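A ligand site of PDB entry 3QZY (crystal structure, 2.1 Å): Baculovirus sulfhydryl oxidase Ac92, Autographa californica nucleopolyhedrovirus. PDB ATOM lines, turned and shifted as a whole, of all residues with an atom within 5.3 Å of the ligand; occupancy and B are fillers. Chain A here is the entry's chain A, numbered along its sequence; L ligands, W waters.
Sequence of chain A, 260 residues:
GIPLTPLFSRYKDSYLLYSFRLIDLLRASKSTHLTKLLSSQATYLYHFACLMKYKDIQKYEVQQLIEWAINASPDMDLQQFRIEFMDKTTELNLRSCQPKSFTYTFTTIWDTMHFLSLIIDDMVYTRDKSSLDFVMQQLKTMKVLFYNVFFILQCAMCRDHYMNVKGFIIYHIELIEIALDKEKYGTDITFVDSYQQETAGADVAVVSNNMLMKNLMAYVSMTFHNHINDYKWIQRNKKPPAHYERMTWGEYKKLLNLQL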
ATOM      1  N   LEU A   7      22.529  -0.214   6.379  1.00  0.00           N
ATOM      2  CA  LEU A   7      21.540   0.260   5.424  1.00  0.00           C
ATOM      3  C   LEU A   7      22.228   0.567   4.096  1.00  0.00           C
ATOM      4  O   LEU A   7      21.700   0.245   3.026  1.00  0.00           O
ATOM      5  CB  LEU A   7      20.815   1.503   5.953  1.00  0.00           C
ATOM      6  CG  LEU A   7      19.679   2.109   5.109  1.00  0.00           C
ATOM      7  CD1 LEU A   7      18.513   1.143   5.022  1.00  0.00           C
ATOM      8  CD2 LEU A   7      19.232   3.430   5.732  1.00  0.00           C
ATOM      9  N   ARG A  10      22.780  -2.491   2.150  1.00  0.00           N
ATOM     10  CA  ARG A  10      21.563  -3.001   1.539  1.00  0.00           C
ATOM     11  C   ARG A  10      21.319  -2.168   0.267  1.00  0.00           C
ATOM     12  O   ARG A  10      20.853  -2.693  -0.745  1.00  0.00           O
ATOM     13  CB  ARG A  10      20.383  -2.850   2.508  1.00  0.00           C
ATOM     14  CG  ARG A  10      19.208  -3.749   2.182  1.00  0.00           C
ATOM     15  CD  ARG A  10      18.020  -3.422   3.063  1.00  0.00           C
ATOM     16  NE  ARG A  10      17.427  -2.129   2.744  1.00  0.00           N
ATOM     17  CZ  ARG A  10      16.461  -1.554   3.451  1.00  0.00           C
ATOM     18  NH1 ARG A  10      15.992  -2.153   4.537  1.00  0.00           N
ATOM     19  NH2 ARG A  10      15.964  -0.379   3.091  1.00  0.00           N
ATOM     20  N   TYR A  11      21.638  -0.879   0.339  1.00  0.00           N
ATOM     21  CA  TYR A  11      21.483   0.040  -0.790  1.00  0.00           C
ATOM     22  C   TYR A  11      22.376  -0.420  -1.937  1.00  0.00           C
ATOM     23  O   TYR A  11      21.949  -0.466  -3.092  1.00  0.00           O
ATOM     24  CB  TYR A  11      21.896   1.466  -0.406  1.00  0.00           C
ATOM     25  CG  TYR A  11      20.873   2.297   0.364  1.00  0.00           C
ATOM     26  CD1 TYR A  11      19.709   1.725   0.883  1.00  0.00           C
ATOM     27  CD2 TYR A  11      21.084   3.662   0.576  1.00  0.00           C
ATOM     28  CE1 TYR A  11      18.787   2.491   1.603  1.00  0.00           C
ATOM     29  CE2 TYR A  11      20.177   4.433   1.286  1.00  0.00           C
ATOM     30  CZ  TYR A  11      19.035   3.839   1.795  1.00  0.00           C
ATOM     31  OH  TYR A  11      18.137   4.627   2.495  1.00  0.00           O
ATOM     32  N   PHE A 106       9.583  -3.046  -3.790  1.00  0.00           N
ATOM     33  CA  PHE A 106       9.563  -1.587  -3.810  1.00  0.00           C
ATOM     34  C   PHE A 106      10.774  -1.066  -3.069  1.00  0.00           C
ATOM     35  O   PHE A 106      11.303  -0.004  -3.398  1.00  0.00           O
ATOM     36  CB  PHE A 106       8.314  -1.055  -3.097  1.00  0.00           C
ATOM     37  CG  PHE A 106       7.064  -1.158  -3.913  1.00  0.00           C
ATOM     38  CD1 PHE A 106       6.946  -0.450  -5.115  1.00  0.00           C
ATOM     39  CD2 PHE A 106       5.995  -1.937  -3.486  1.00  0.00           C
ATOM     40  CE1 PHE A 106       5.780  -0.520  -5.869  1.00  0.00           C
ATOM     41  CE2 PHE A 106       4.816  -2.012  -4.231  1.00  0.00           C
ATOM     42  CZ  PHE A 106       4.711  -1.299  -5.432  1.00  0.00           C
ATOM     43  N   THR A 107      11.202  -1.810  -2.054  1.00  0.00           N
ATOM     44  CA  THR A 107      12.356  -1.417  -1.265  1.00  0.00           C
ATOM     45  C   THR A 107      13.614  -1.420  -2.131  1.00  0.00           C
ATOM     46  O   THR A 107      14.558  -0.680  -1.870  1.00  0.00           O
ATOM     47  CB  THR A 107      12.568  -2.356  -0.076  1.00  0.00           C
ATOM     48  OG1 THR A 107      11.306  -2.663   0.526  1.00  0.00           O
ATOM     49  CG2 THR A 107      13.444  -1.697   0.954  1.00  0.00           C
ATOM     50  N   ILE A 109      13.713  -0.572  -5.299  1.00  0.00           N
ATOM     51  CA  ILE A 109      13.665   0.679  -6.062  1.00  0.00           C
ATOM     52  C   ILE A 109      13.941   1.872  -5.162  1.00  0.00           C
ATOM     53  O   ILE A 109      14.726   2.755  -5.531  1.00  0.00           O
ATOM     54  CB  ILE A 109      12.303   0.836  -6.766  1.00  0.00           C
ATOM     55  CG1 ILE A 109      12.033  -0.430  -7.606  1.00  0.00           C
ATOM     56  CG2 ILE A 109      12.337   2.047  -7.719  1.00  0.00           C
ATOM     57  CD1 ILE A 109      10.710  -0.395  -8.361  1.00  0.00           C
ATOM     58  N   TRP A 110      13.329   1.901  -3.979  1.00  0.00           N
ATOM     59  CA  TRP A 110      13.545   2.979  -3.031  1.00  0.00           C
ATOM     60  C   TRP A 110      15.018   3.052  -2.623  1.00  0.00           C
ATOM     61  O   TRP A 110      15.623   4.111  -2.601  1.00  0.00           O
ATOM     62  CB  TRP A 110      12.659   2.789  -1.794  1.00  0.00           C
ATOM     63  CG  TRP A 110      11.265   3.382  -1.971  1.00  0.00           C
ATOM     64  CD1 TRP A 110      10.063   2.757  -1.764  1.00  0.00           C
ATOM     65  CD2 TRP A 110      10.951   4.710  -2.417  1.00  0.00           C
ATOM     66  NE1 TRP A 110       9.025   3.616  -2.054  1.00  0.00           N
ATOM     67  CE2 TRP A 110       9.535   4.814  -2.452  1.00  0.00           C
ATOM     68  CE3 TRP A 110      11.723   5.825  -2.782  1.00  0.00           C
ATOM     69  CZ2 TRP A 110       8.882   5.993  -2.843  1.00  0.00           C
ATOM     70  CZ3 TRP A 110      11.082   6.986  -3.174  1.00  0.00           C
ATOM     71  CH2 TRP A 110       9.662   7.059  -3.199  1.00  0.00           C
ATOM     72  N   ASP A 111      15.587   1.885  -2.303  1.00  0.00           N
ATOM     73  CA  ASP A 111      16.990   1.803  -1.918  1.00  0.00           C
ATOM     74  C   ASP A 111      17.882   2.305  -3.061  1.00  0.00           C
ATOM     75  O   ASP A 111      18.901   2.949  -2.820  1.00  0.00           O
ATOM     76  CB  ASP A 111      17.361   0.345  -1.613  1.00  0.00           C
ATOM     77  CG  ASP A 111      17.010  -0.052  -0.183  1.00  0.00           C
ATOM     78  OD1 ASP A 111      15.958   0.381   0.331  1.00  0.00           O
ATOM     79  OD2 ASP A 111      17.791  -0.816   0.416  1.00  0.00           O
ATOM     80  N   MET A 113      17.004   4.477  -5.371  1.00  0.00           N
ATOM     81  CA  MET A 113      16.828   5.919  -5.473  1.00  0.00           C
ATOM     82  C   MET A 113      17.579   6.642  -4.344  1.00  0.00           C
ATOM     83  O   MET A 113      18.151   7.701  -4.553  1.00  0.00           O
ATOM     84  CB  MET A 113      15.324   6.283  -5.455  1.00  0.00           C
ATOM     85  CG  MET A 113      14.546   5.723  -6.662  1.00  0.00           C
ATOM     86  SD  MET A 113      12.737   5.896  -6.550  1.00  0.00           S
ATOM     87  CE  MET A 113      12.558   7.716  -6.827  1.00  0.00           C
ATOM     88  N   HIS A 114      17.566   6.071  -3.142  1.00  0.00           N
ATOM     89  CA  HIS A 114      18.292   6.705  -2.035  1.00  0.00           C
ATOM     90  C   HIS A 114      19.791   6.564  -2.320  1.00  0.00           C
ATOM     91  O   HIS A 114      20.557   7.502  -2.138  1.00  0.00           O
ATOM     92  CB  HIS A 114      17.923   6.059  -0.688  1.00  0.00           C
ATOM     93  CG  HIS A 114      16.483   6.270  -0.311  1.00  0.00           C
ATOM     94  ND1 HIS A 114      15.898   7.518  -0.301  1.00  0.00           N
ATOM     95  CD2 HIS A 114      15.498   5.393  -0.015  1.00  0.00           C
ATOM     96  CE1 HIS A 114      14.613   7.399  -0.027  1.00  0.00           C
ATOM     97  NE2 HIS A 114      14.340   6.114   0.152  1.00  0.00           N
ATOM     98  N   VAL A 149      12.721   5.849 -13.983  1.00  0.00           N
ATOM     99  CA  VAL A 149      12.472   4.852 -12.969  1.00  0.00           C
ATOM    100  C   VAL A 149      11.105   4.210 -13.204  1.00  0.00           C
ATOM    101  O   VAL A 149      10.837   3.109 -12.732  1.00  0.00           O
ATOM    102  CB  VAL A 149      12.492   5.458 -11.560  1.00  0.00           C
ATOM    103  CG1 VAL A 149      11.966   4.449 -10.550  1.00  0.00           C
ATOM    104  CG2 VAL A 149      13.902   5.859 -11.188  1.00  0.00           C
ATOM    105  N   CYS A 155       3.212  -1.846 -10.868  1.00  0.00           N
ATOM    106  CA  CYS A 155       2.131  -1.060 -10.309  1.00  0.00           C
ATOM    107  C   CYS A 155       1.811   0.145 -11.196  1.00  0.00           C
ATOM    108  O   CYS A 155       2.460   1.180 -11.115  1.00  0.00           O
ATOM    109  CB  CYS A 155       2.480  -0.583  -8.898  1.00  0.00           C
ATOM    110  SG  CYS A 155       1.290   0.575  -8.176  1.00  0.00           S
ATOM    111  N   MET A 157      -0.516   2.207 -10.994  1.00  0.00           N
ATOM    112  CA  MET A 157      -0.853   3.353 -10.162  1.00  0.00           C
ATOM    113  C   MET A 157       0.399   4.120  -9.747  1.00  0.00           C
ATOM    114  O   MET A 157       0.459   5.345  -9.840  1.00  0.00           O
ATOM    115  CB  MET A 157      -1.632   2.915  -8.927  1.00  0.00           C
ATOM    116  CG  MET A 157      -1.781   3.990  -7.864  1.00  0.00           C
ATOM    117  SD  MET A 157      -2.727   3.432  -6.432  1.00  0.00           S
ATOM    118  CE  MET A 157      -1.681   2.098  -5.848  1.00  0.00           C
ATOM    119  N   CYS A 158       1.411   3.384  -9.296  1.00  0.00           N
ATOM    120  CA  CYS A 158       2.668   3.989  -8.863  1.00  0.00           C
ATOM    121  C   CYS A 158       3.337   4.733 -10.015  1.00  0.00           C
ATOM    122  O   CYS A 158       3.852   5.837  -9.834  1.00  0.00           O
ATOM    123  CB  CYS A 158       3.608   2.927  -8.297  1.00  0.00           C
ATOM    124  SG  CYS A 158       2.891   1.900  -6.999  1.00  0.00           S
ATOM    125  N   HIS A 161       1.555   8.097 -10.679  1.00  0.00           N
ATOM    126  CA  HIS A 161       1.874   9.051  -9.642  1.00  0.00           C
ATOM    127  C   HIS A 161       3.310   9.541  -9.839  1.00  0.00           C
ATOM    128  O   HIS A 161       3.561  10.744  -9.929  1.00  0.00           O
ATOM    129  CB  HIS A 161       1.745   8.413  -8.262  1.00  0.00           C
ATOM    130  CG  HIS A 161       1.902   9.382  -7.127  1.00  0.00           C
ATOM    131  ND1 HIS A 161       1.977   8.977  -5.811  1.00  0.00           N
ATOM    132  CD2 HIS A 161       1.946  10.727  -7.108  1.00  0.00           C
ATOM    133  CE1 HIS A 161       2.073  10.042  -5.025  1.00  0.00           C
ATOM    134  NE2 HIS A 161       2.048  11.122  -5.791  1.00  0.00           N
ATOM    135  N   TYR A 162       4.251   8.604  -9.941  1.00  0.00           N
ATOM    136  CA  TYR A 162       5.653   8.986 -10.120  1.00  0.00           C
ATOM    137  C   TYR A 162       5.849   9.903 -11.325  1.00  0.00           C
ATOM    138  O   TYR A 162       6.595  10.887 -11.243  1.00  0.00           O
ATOM    139  CB  TYR A 162       6.562   7.751 -10.276  1.00  0.00           C
ATOM    140  CG  TYR A 162       8.033   8.094 -10.275  1.00  0.00           C
ATOM    141  CD1 TYR A 162       8.648   8.583  -9.141  1.00  0.00           C
ATOM    142  CD2 TYR A 162       8.807   7.945 -11.428  1.00  0.00           C
ATOM    143  CE1 TYR A 162       9.998   8.911  -9.121  1.00  0.00           C
ATOM    144  CE2 TYR A 162      10.161   8.260 -11.428  1.00  0.00           C
ATOM    145  CZ  TYR A 162      10.749   8.740 -10.264  1.00  0.00           C
ATOM    146  OH  TYR A 162      12.085   9.063 -10.235  1.00  0.00           O
ATOM    147  N   SER A 221      15.223  12.996  -1.313  1.00  0.00           N
ATOM    148  CA  SER A 221      14.691  11.665  -1.587  1.00  0.00           C
ATOM    149  C   SER A 221      13.958  11.123  -0.363  1.00  0.00           C
ATOM    150  O   SER A 221      12.964  10.418  -0.484  1.00  0.00           O
ATOM    151  CB  SER A 221      15.802  10.703  -2.038  1.00  0.00           C
ATOM    152  OG  SER A 221      16.685  10.350  -0.983  1.00  0.00           O
ATOM    153  N   MET A 222      14.427  11.462   0.837  1.00  0.00           N
ATOM    154  CA  MET A 222      13.732  10.991   2.023  1.00  0.00           C
ATOM    155  C   MET A 222      12.360  11.670   2.067  1.00  0.00           C
ATOM    156  O   MET A 222      11.332  11.033   2.286  1.00  0.00           O
ATOM    157  CB  MET A 222      14.509  11.359   3.287  1.00  0.00           C
ATOM    158  CG  MET A 222      13.796  10.918   4.573  1.00  0.00           C
ATOM    159  SD  MET A 222      14.371  11.784   6.042  1.00  0.00           S
ATOM    160  CE  MET A 222      13.413  13.266   5.911  1.00  0.00           C
ATOM    161  N   THR A 223      12.338  12.976   1.834  1.00  0.00           N
ATOM    162  CA  THR A 223      11.094  13.724   1.830  1.00  0.00           C
ATOM    163  C   THR A 223      10.163  13.197   0.732  1.00  0.00           C
ATOM    164  O   THR A 223       8.978  12.947   0.985  1.00  0.00           O
ATOM    165  CB  THR A 223      11.385  15.215   1.594  1.00  0.00           C
ATOM    166  OG1 THR A 223      12.512  15.599   2.393  1.00  0.00           O
ATOM    167  CG2 THR A 223      10.192  16.064   1.973  1.00  0.00           C
ATOM    168  N   PHE A 224      10.692  13.010  -0.474  1.00  0.00           N
ATOM    169  CA  PHE A 224       9.896  12.502  -1.601  1.00  0.00           C
ATOM    170  C   PHE A 224       9.285  11.155  -1.226  1.00  0.00           C
ATOM    171  O   PHE A 224       8.105  10.890  -1.474  1.00  0.00           O
ATOM    172  CB  PHE A 224      10.766  12.339  -2.843  1.00  0.00           C
ATOM    173  CG  PHE A 224       9.995  11.877  -4.079  1.00  0.00           C
ATOM    174  CD1 PHE A 224       9.295  12.794  -4.874  1.00  0.00           C
ATOM    175  CD2 PHE A 224      10.027  10.544  -4.477  1.00  0.00           C
ATOM    176  CE1 PHE A 224       8.637  12.374  -6.048  1.00  0.00           C
ATOM    177  CE2 PHE A 224       9.382  10.128  -5.650  1.00  0.00           C
ATOM    178  CZ  PHE A 224       8.692  11.040  -6.426  1.00  0.00           C
ATOM    179  N   HIS A 225      10.104  10.292  -0.629  1.00  0.00           N
ATOM    180  CA  HIS A 225       9.680   8.957  -0.202  1.00  0.00           C
ATOM    181  C   HIS A 225       8.495   9.055   0.776  1.00  0.00           C
ATOM    182  O   HIS A 225       7.479   8.374   0.595  1.00  0.00           O
ATOM    183  CB  HIS A 225      10.873   8.202   0.411  1.00  0.00           C
ATOM    184  CG  HIS A 225      10.641   6.737   0.598  1.00  0.00           C
ATOM    185  ND1 HIS A 225      11.679   5.835   0.748  1.00  0.00           N
ATOM    186  CD2 HIS A 225       9.509   6.009   0.695  1.00  0.00           C
ATOM    187  CE1 HIS A 225      11.184   4.622   0.915  1.00  0.00           C
ATOM    188  NE2 HIS A 225       9.871   4.706   0.891  1.00  0.00           N
ATOM    189  N   ASN A 226       8.623   9.883   1.809  1.00  0.00           N
ATOM    190  CA  ASN A 226       7.533  10.033   2.779  1.00  0.00           C
ATOM    191  C   ASN A 226       6.249  10.531   2.141  1.00  0.00           C
ATOM    192  O   ASN A 226       5.157  10.072   2.492  1.00  0.00           O
ATOM    193  CB  ASN A 226       7.918  11.006   3.897  1.00  0.00           C
ATOM    194  CG  ASN A 226       8.736  10.337   4.987  1.00  0.00           C
ATOM    195  OD1 ASN A 226       8.527   9.152   5.298  1.00  0.00           O
ATOM    196  ND2 ASN A 226       9.659  11.082   5.588  1.00  0.00           N
ATOM    197  N   ILE A 228       5.238  10.155  -0.997  1.00  0.00           N
ATOM    198  CA  ILE A 228       4.632   9.088  -1.769  1.00  0.00           C
ATOM    199  C   ILE A 228       3.805   8.172  -0.861  1.00  0.00           C
ATOM    200  O   ILE A 228       2.699   7.746  -1.229  1.00  0.00           O
ATOM    201  CB  ILE A 228       5.690   8.238  -2.498  1.00  0.00           C
ATOM    202  CG1 ILE A 228       6.445   9.081  -3.528  1.00  0.00           C
ATOM    203  CG2 ILE A 228       5.013   7.060  -3.192  1.00  0.00           C
ATOM    204  CD1 ILE A 228       5.547   9.835  -4.478  1.00  0.00           C
ATOM    205  N   ASN A 229       4.344   7.875   0.312  1.00  0.00           N
ATOM    206  CA  ASN A 229       3.639   7.019   1.272  1.00  0.00           C
ATOM    207  C   ASN A 229       2.462   7.752   1.919  1.00  0.00           C
ATOM    208  O   ASN A 229       1.447   7.139   2.259  1.00  0.00           O
ATOM    209  CB  ASN A 229       4.599   6.490   2.346  1.00  0.00           C
ATOM    210  CG  ASN A 229       5.478   5.345   1.840  1.00  0.00           C
ATOM    211  OD1 ASN A 229       5.161   4.696   0.847  1.00  0.00           O
ATOM    212  ND2 ASN A 229       6.578   5.078   2.539  1.00  0.00           N
ATOM    213  N   LYS A 232      -0.470   7.681  -0.806  1.00  0.00           N
ATOM    214  CA  LYS A 232      -1.108   6.407  -1.131  1.00  0.00           C
ATOM    215  C   LYS A 232      -2.393   6.144  -0.360  1.00  0.00           C
ATOM    216  O   LYS A 232      -3.276   5.432  -0.840  1.00  0.00           O
ATOM    217  CB  LYS A 232      -0.121   5.237  -0.936  1.00  0.00           C
ATOM    218  CG  LYS A 232       0.322   4.975   0.495  1.00  0.00           C
ATOM    219  CD  LYS A 232       1.310   3.785   0.510  1.00  0.00           C
ATOM    220  CE  LYS A 232       1.834   3.502   1.913  1.00  0.00           C
ATOM    221  NZ  LYS A 232       2.975   2.537   1.912  1.00  0.00           N
ATOM    222  N   GLN A 235      -4.925   7.737  -2.397  1.00  0.00           N
ATOM    223  CA  GLN A 235      -5.224   6.969  -3.601  1.00  0.00           C
ATOM    224  C   GLN A 235      -6.127   5.798  -3.248  1.00  0.00           C
ATOM    225  O   GLN A 235      -7.087   5.494  -3.953  1.00  0.00           O
ATOM    226  CB  GLN A 235      -3.941   6.439  -4.224  1.00  0.00           C
ATOM    227  CG  GLN A 235      -3.007   7.495  -4.779  1.00  0.00           C
ATOM    228  CD  GLN A 235      -1.669   6.898  -5.202  1.00  0.00           C
ATOM    229  OE1 GLN A 235      -0.971   6.298  -4.402  1.00  0.00           O
ATOM    230  NE2 GLN A 235      -1.320   7.078  -6.475  1.00  0.00           N
ATOM    231  N   ARG A 236      -5.796   5.127  -2.143  1.00  0.00           N
ATOM    232  CA  ARG A 236      -6.535   3.969  -1.668  1.00  0.00           C
ATOM    233  C   ARG A 236      -7.738   4.373  -0.826  1.00  0.00           C
ATOM    234  O   ARG A 236      -8.580   3.533  -0.497  1.00  0.00           O
ATOM    235  CB  ARG A 236      -5.615   3.082  -0.839  1.00  0.00           C
ATOM    236  CG  ARG A 236      -4.273   2.793  -1.478  1.00  0.00           C
ATOM    237  CD  ARG A 236      -3.370   2.047  -0.498  1.00  0.00           C
ATOM    238  NE  ARG A 236      -2.078   1.727  -1.097  1.00  0.00           N
ATOM    239  CZ  ARG A 236      -1.158   0.969  -0.507  1.00  0.00           C
ATOM    240  NH1 ARG A 236      -1.388   0.456   0.693  1.00  0.00           N
ATOM    241  NH2 ARG A 236      -0.002   0.732  -1.117  1.00  0.00           N
ATOM    242  N   MET A 247       9.613   8.321   8.540  1.00  0.00           N
ATOM    243  CA  MET A 247      11.045   8.570   8.570  1.00  0.00           C
ATOM    244  C   MET A 247      11.340  10.050   8.814  1.00  0.00           C
ATOM    245  O   MET A 247      10.776  10.927   8.149  1.00  0.00           O
ATOM    246  CB  MET A 247      11.672   8.141   7.231  1.00  0.00           C
ATOM    247  CG  MET A 247      13.184   8.305   7.140  1.00  0.00           C
ATOM    248  SD  MET A 247      14.070   7.337   8.387  1.00  0.00           S
ATOM    249  CE  MET A 247      13.821   5.683   7.761  1.00  0.00           C
ATOM    250  N   TYR A 252      17.203   9.361   9.951  1.00  0.00           N
ATOM    251  CA  TYR A 252      17.771   8.928   8.682  1.00  0.00           C
ATOM    252  C   TYR A 252      19.268   9.213   8.613  1.00  0.00           C
ATOM    253  O   TYR A 252      20.029   8.380   8.130  1.00  0.00           O
ATOM    254  CB  TYR A 252      17.080   9.644   7.524  1.00  0.00           C
ATOM    255  CG  TYR A 252      17.346   9.045   6.168  1.00  0.00           C
ATOM    256  CD1 TYR A 252      16.922   7.748   5.855  1.00  0.00           C
ATOM    257  CD2 TYR A 252      17.995   9.773   5.165  1.00  0.00           C
ATOM    258  CE1 TYR A 252      17.125   7.202   4.590  1.00  0.00           C
ATOM    259  CE2 TYR A 252      18.198   9.228   3.890  1.00  0.00           C
ATOM    260  CZ  TYR A 252      17.761   7.948   3.617  1.00  0.00           C
ATOM    261  OH  TYR A 252      17.937   7.416   2.362  1.00  0.00           O
HETATM  262  P1  LIG L   1       8.575   1.432   2.561  1.00  0.00           P
HETATM  263  O1  LIG L   1       8.146   2.488   3.511  1.00  0.00           O
HETATM  264  O2  LIG L   1       8.581   1.774   1.116  1.00  0.00           O
HETATM  265  O3  LIG L   1      10.032   0.916   2.891  1.00  0.00           O
HETATM  266  C1  LIG L   1      11.174   1.423   2.221  1.00  0.00           C
HETATM  267  C2  LIG L   1      12.407   1.195   3.082  1.00  0.00           C
HETATM  268  O4  LIG L   1      13.072   2.434   3.317  1.00  0.00           O
HETATM  269  C3  LIG L   1      12.247   0.562   4.482  1.00  0.00           C
HETATM  270  O5  LIG L   1      13.440  -0.175   4.735  1.00  0.00           O
HETATM  271  C4  LIG L   1      12.089   1.725   5.386  1.00  0.00           C
HETATM  272  O6  LIG L   1      12.669   1.676   6.652  1.00  0.00           O
HETATM  273  C5  LIG L   1      12.778   2.914   4.630  1.00  0.00           C
HETATM  274  N1  LIG L   1      12.023   4.118   4.518  1.00  0.00           N
HETATM  275  C6  LIG L   1      10.644   4.378   4.776  1.00  0.00           C
HETATM  276  N2  LIG L   1      10.276   5.585   4.509  1.00  0.00           N
HETATM  277  C7  LIG L   1      11.445   6.231   4.101  1.00  0.00           C
HETATM  278  C8  LIG L   1      11.725   7.572   3.753  1.00  0.00           C
HETATM  279  N3  LIG L   1      10.781   8.502   3.675  1.00  0.00           N
HETATM  280  N4  LIG L   1      13.033   7.883   3.402  1.00  0.00           N
HETATM  281  C9  LIG L   1      13.979   6.911   3.279  1.00  0.00           C
HETATM  282  N5  LIG L   1      13.779   5.551   3.588  1.00  0.00           N
HETATM  283  C10 LIG L   1      12.428   5.373   4.060  1.00  0.00           C
HETATM  284  N6  LIG L   1       2.550   2.824  -3.469  1.00  0.00           N
HETATM  285  C11 LIG L   1       1.237   3.228  -3.689  1.00  0.00           C
HETATM  286  O7  LIG L   1       0.274   2.651  -3.128  1.00  0.00           O
HETATM  287  N7  LIG L   1       0.984   4.240  -4.618  1.00  0.00           N
HETATM  288  C12 LIG L   1       1.979   4.918  -5.387  1.00  0.00           C
HETATM  289  O8  LIG L   1       1.628   5.810  -6.229  1.00  0.00           O
HETATM  290  C13 LIG L   1       3.269   4.492  -5.168  1.00  0.00           C
HETATM  291  N8  LIG L   1       4.303   5.137  -5.958  1.00  0.00           N
HETATM  292  C14 LIG L   1       5.632   4.658  -5.769  1.00  0.00           C
HETATM  293  C15 LIG L   1       6.686   5.146  -6.580  1.00  0.00           C
HETATM  294  C16 LIG L   1       8.025   4.663  -6.502  1.00  0.00           C
HETATM  295  C17 LIG L   1       9.123   5.300  -7.370  1.00  0.00           C
HETATM  296  C18 LIG L   1       8.299   3.584  -5.593  1.00  0.00           C
HETATM  297  C19 LIG L   1       9.688   2.983  -5.436  1.00  0.00           C
HETATM  298  C20 LIG L   1       7.280   3.010  -4.843  1.00  0.00           C
HETATM  299  C21 LIG L   1       5.982   3.571  -4.810  1.00  0.00           C
HETATM  300  N9  LIG L   1       4.838   3.040  -4.010  1.00  0.00           N
HETATM  301  C22 LIG L   1       3.543   3.457  -4.219  1.00  0.00           C
HETATM  302  C23 LIG L   1       5.126   2.009  -3.051  1.00  0.00           C
HETATM  303  C24 LIG L   1       5.174   2.453  -1.614  1.00  0.00           C
HETATM  304  O9  LIG L   1       5.877   3.721  -1.579  1.00  0.00           O
HETATM  305  C25 LIG L   1       5.848   1.511  -0.649  1.00  0.00           C
HETATM  306  O10 LIG L   1       7.146   1.117  -1.060  1.00  0.00           O
HETATM  307  C26 LIG L   1       5.127   0.190  -0.366  1.00  0.00           C
HETATM  308  O11 LIG L   1       3.697   0.525  -0.248  1.00  0.00           O
HETATM  309  C27 LIG L   1       5.580  -0.548   0.839  1.00  0.00           C
HETATM  310  O12 LIG L   1       5.283   0.185   2.026  1.00  0.00           O
HETATM  311  P2  LIG L   1       6.151   0.039   3.334  1.00  0.00           P
HETATM  312  O13 LIG L   1       5.759   1.145   4.205  1.00  0.00           O
HETATM  313  O14 LIG L   1       6.073  -1.366   3.824  1.00  0.00           O
HETATM  314  O15 LIG L   1       7.637   0.215   2.804  1.00  0.00           O
HETATM  315  O   HOH W   1      15.926   3.636   2.996  1.00  0.00           O
HETATM  316  O   HOH W   2      14.482   2.473   0.903  1.00  0.00           O
HETATM  317  O   HOH W   3       0.993   7.711  -3.620  1.00  0.00           O
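The side-chain amide oxygen (OD1) of Asn 229 lies within hydrogen-bond range of an oxygen (O9) of the ligand (2.7 Å).
The guanidinium group of Arg 236 is in hydrogen-bond range of an oxygen (O7) of the ligand, at 2.8 Å.
A nitrogen (N7) of the ligand lies within hydrogen-bond range of the side-chain amide oxygen (OE1) of Gln 235 (2.8 Å).
OD1 of Asn 226 sits at hydrogen-bond distance from N3 of the ligand, 2.9 Å away.
O of Met 222 sits at hydrogen-bond distance from N3 of the ligand (2.9 Å).
An oxygen (O5) of the ligand is in hydrogen-bond range of the guanidinium group (NH2) of Arg 10, 3.0 Å away.
The side-chain amino group (NZ) of Lys 232 lies within salt-bridge range of an oxygen (O13) of the ligand, 3.9 Å away.
The indole nitrogen of Trp 110 sits at hydrogen-bond distance from an oxygen (O9) of the ligand (3.2 Å).
An oxygen (O2) of the ligand sits at hydrogen-bond distance from a ring nitrogen (NE2) of His 225.
O8 of the ligand is in hydrogen-bond range of ND1 of His 161 (3.2 Å).
The side-chain amino group (NZ) of Lys 232 lies within hydrogen-bond range of the side-chain amide oxygen (OD1) of Asn 229 (3.3 Å).
ND2 of Asn 226 lies within hydrogen-bond range of O of Met 247 (2.8 Å).
The guanidinium group of Arg 10 is in salt-bridge range of the side-chain carboxylate of Asp 111, at 2.7 Å.
SG of Cys 158 is disulfide-bonded to SG of Cys 155.
A ring nitrogen (ND1) of His 114 lies close to the side-chain hydroxyl (OH) of Tyr 252, 3.4 Å away.
A ring nitrogen (ND1) of His 114 lies within hydrogen-bond range of the side-chain hydroxyl (OG) of Ser 221 (3.0 Å).
The backbone NH (N) of Met 157 sits close to the side-chain sulfur (SG) of Cys 155.
OH of Tyr 11 lies within hydrogen-bond range of OH of Tyr 252 (2.8 Å).
A nitrogen (N6) of the ligand sits close to the side-chain sulfur (SG) of Cys 158 (3.7 Å).
Phe 106 touches the ligand.
CG2 of Thr 107 touches C2 of the ligand, 3.7 Å away.
Ile 109 touches the ligand.
Met 113 touches the ligand.
His 114 touches the ligand (NE2 to C9, 3.2 Å).
Met 157 touches the ligand (CE to O7, 3.4 Å).
Tyr 162 touches the ligand.
Ile 228 touches the ligand (CG2 to N8, 3.4 Å).
Met 247 touches the ligand (CB to C8, 3.5 Å).
Tyr 252 touches the ligand (CE1 to C9, 3.4 Å).
Hydrophobic or aromatic side chains within 4 Å of the ligand: Phe 106, Ile 109, Trp 110, Met 113, His 114, Met 157, His 161, Tyr 162, Met 222, His 225, Ile 228, Met 247 and Tyr 252.
21 residues have an atom within 4 Å of the ligand: Arg 10, Phe 106, Thr 107, Ile 109, Trp 110, Met 113, His 114, Met 157, Cys 158, His 161, Tyr 162, Met 222, His 225, Asn 226, Ile 228, Asn 229, Lys 232, Gln 235, Arg 236, Met 247 and Tyr 252.
Water W2 bridges the side-chain carboxylate (OD1) of Asp 111 (2.6 Å) and an oxygen (O4) of the ligand (2.8 Å).
Water W1 lies within hydrogen-bond range of OH of Tyr 11 (2.5 Å) and N5 of the ligand (2.9 Å).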
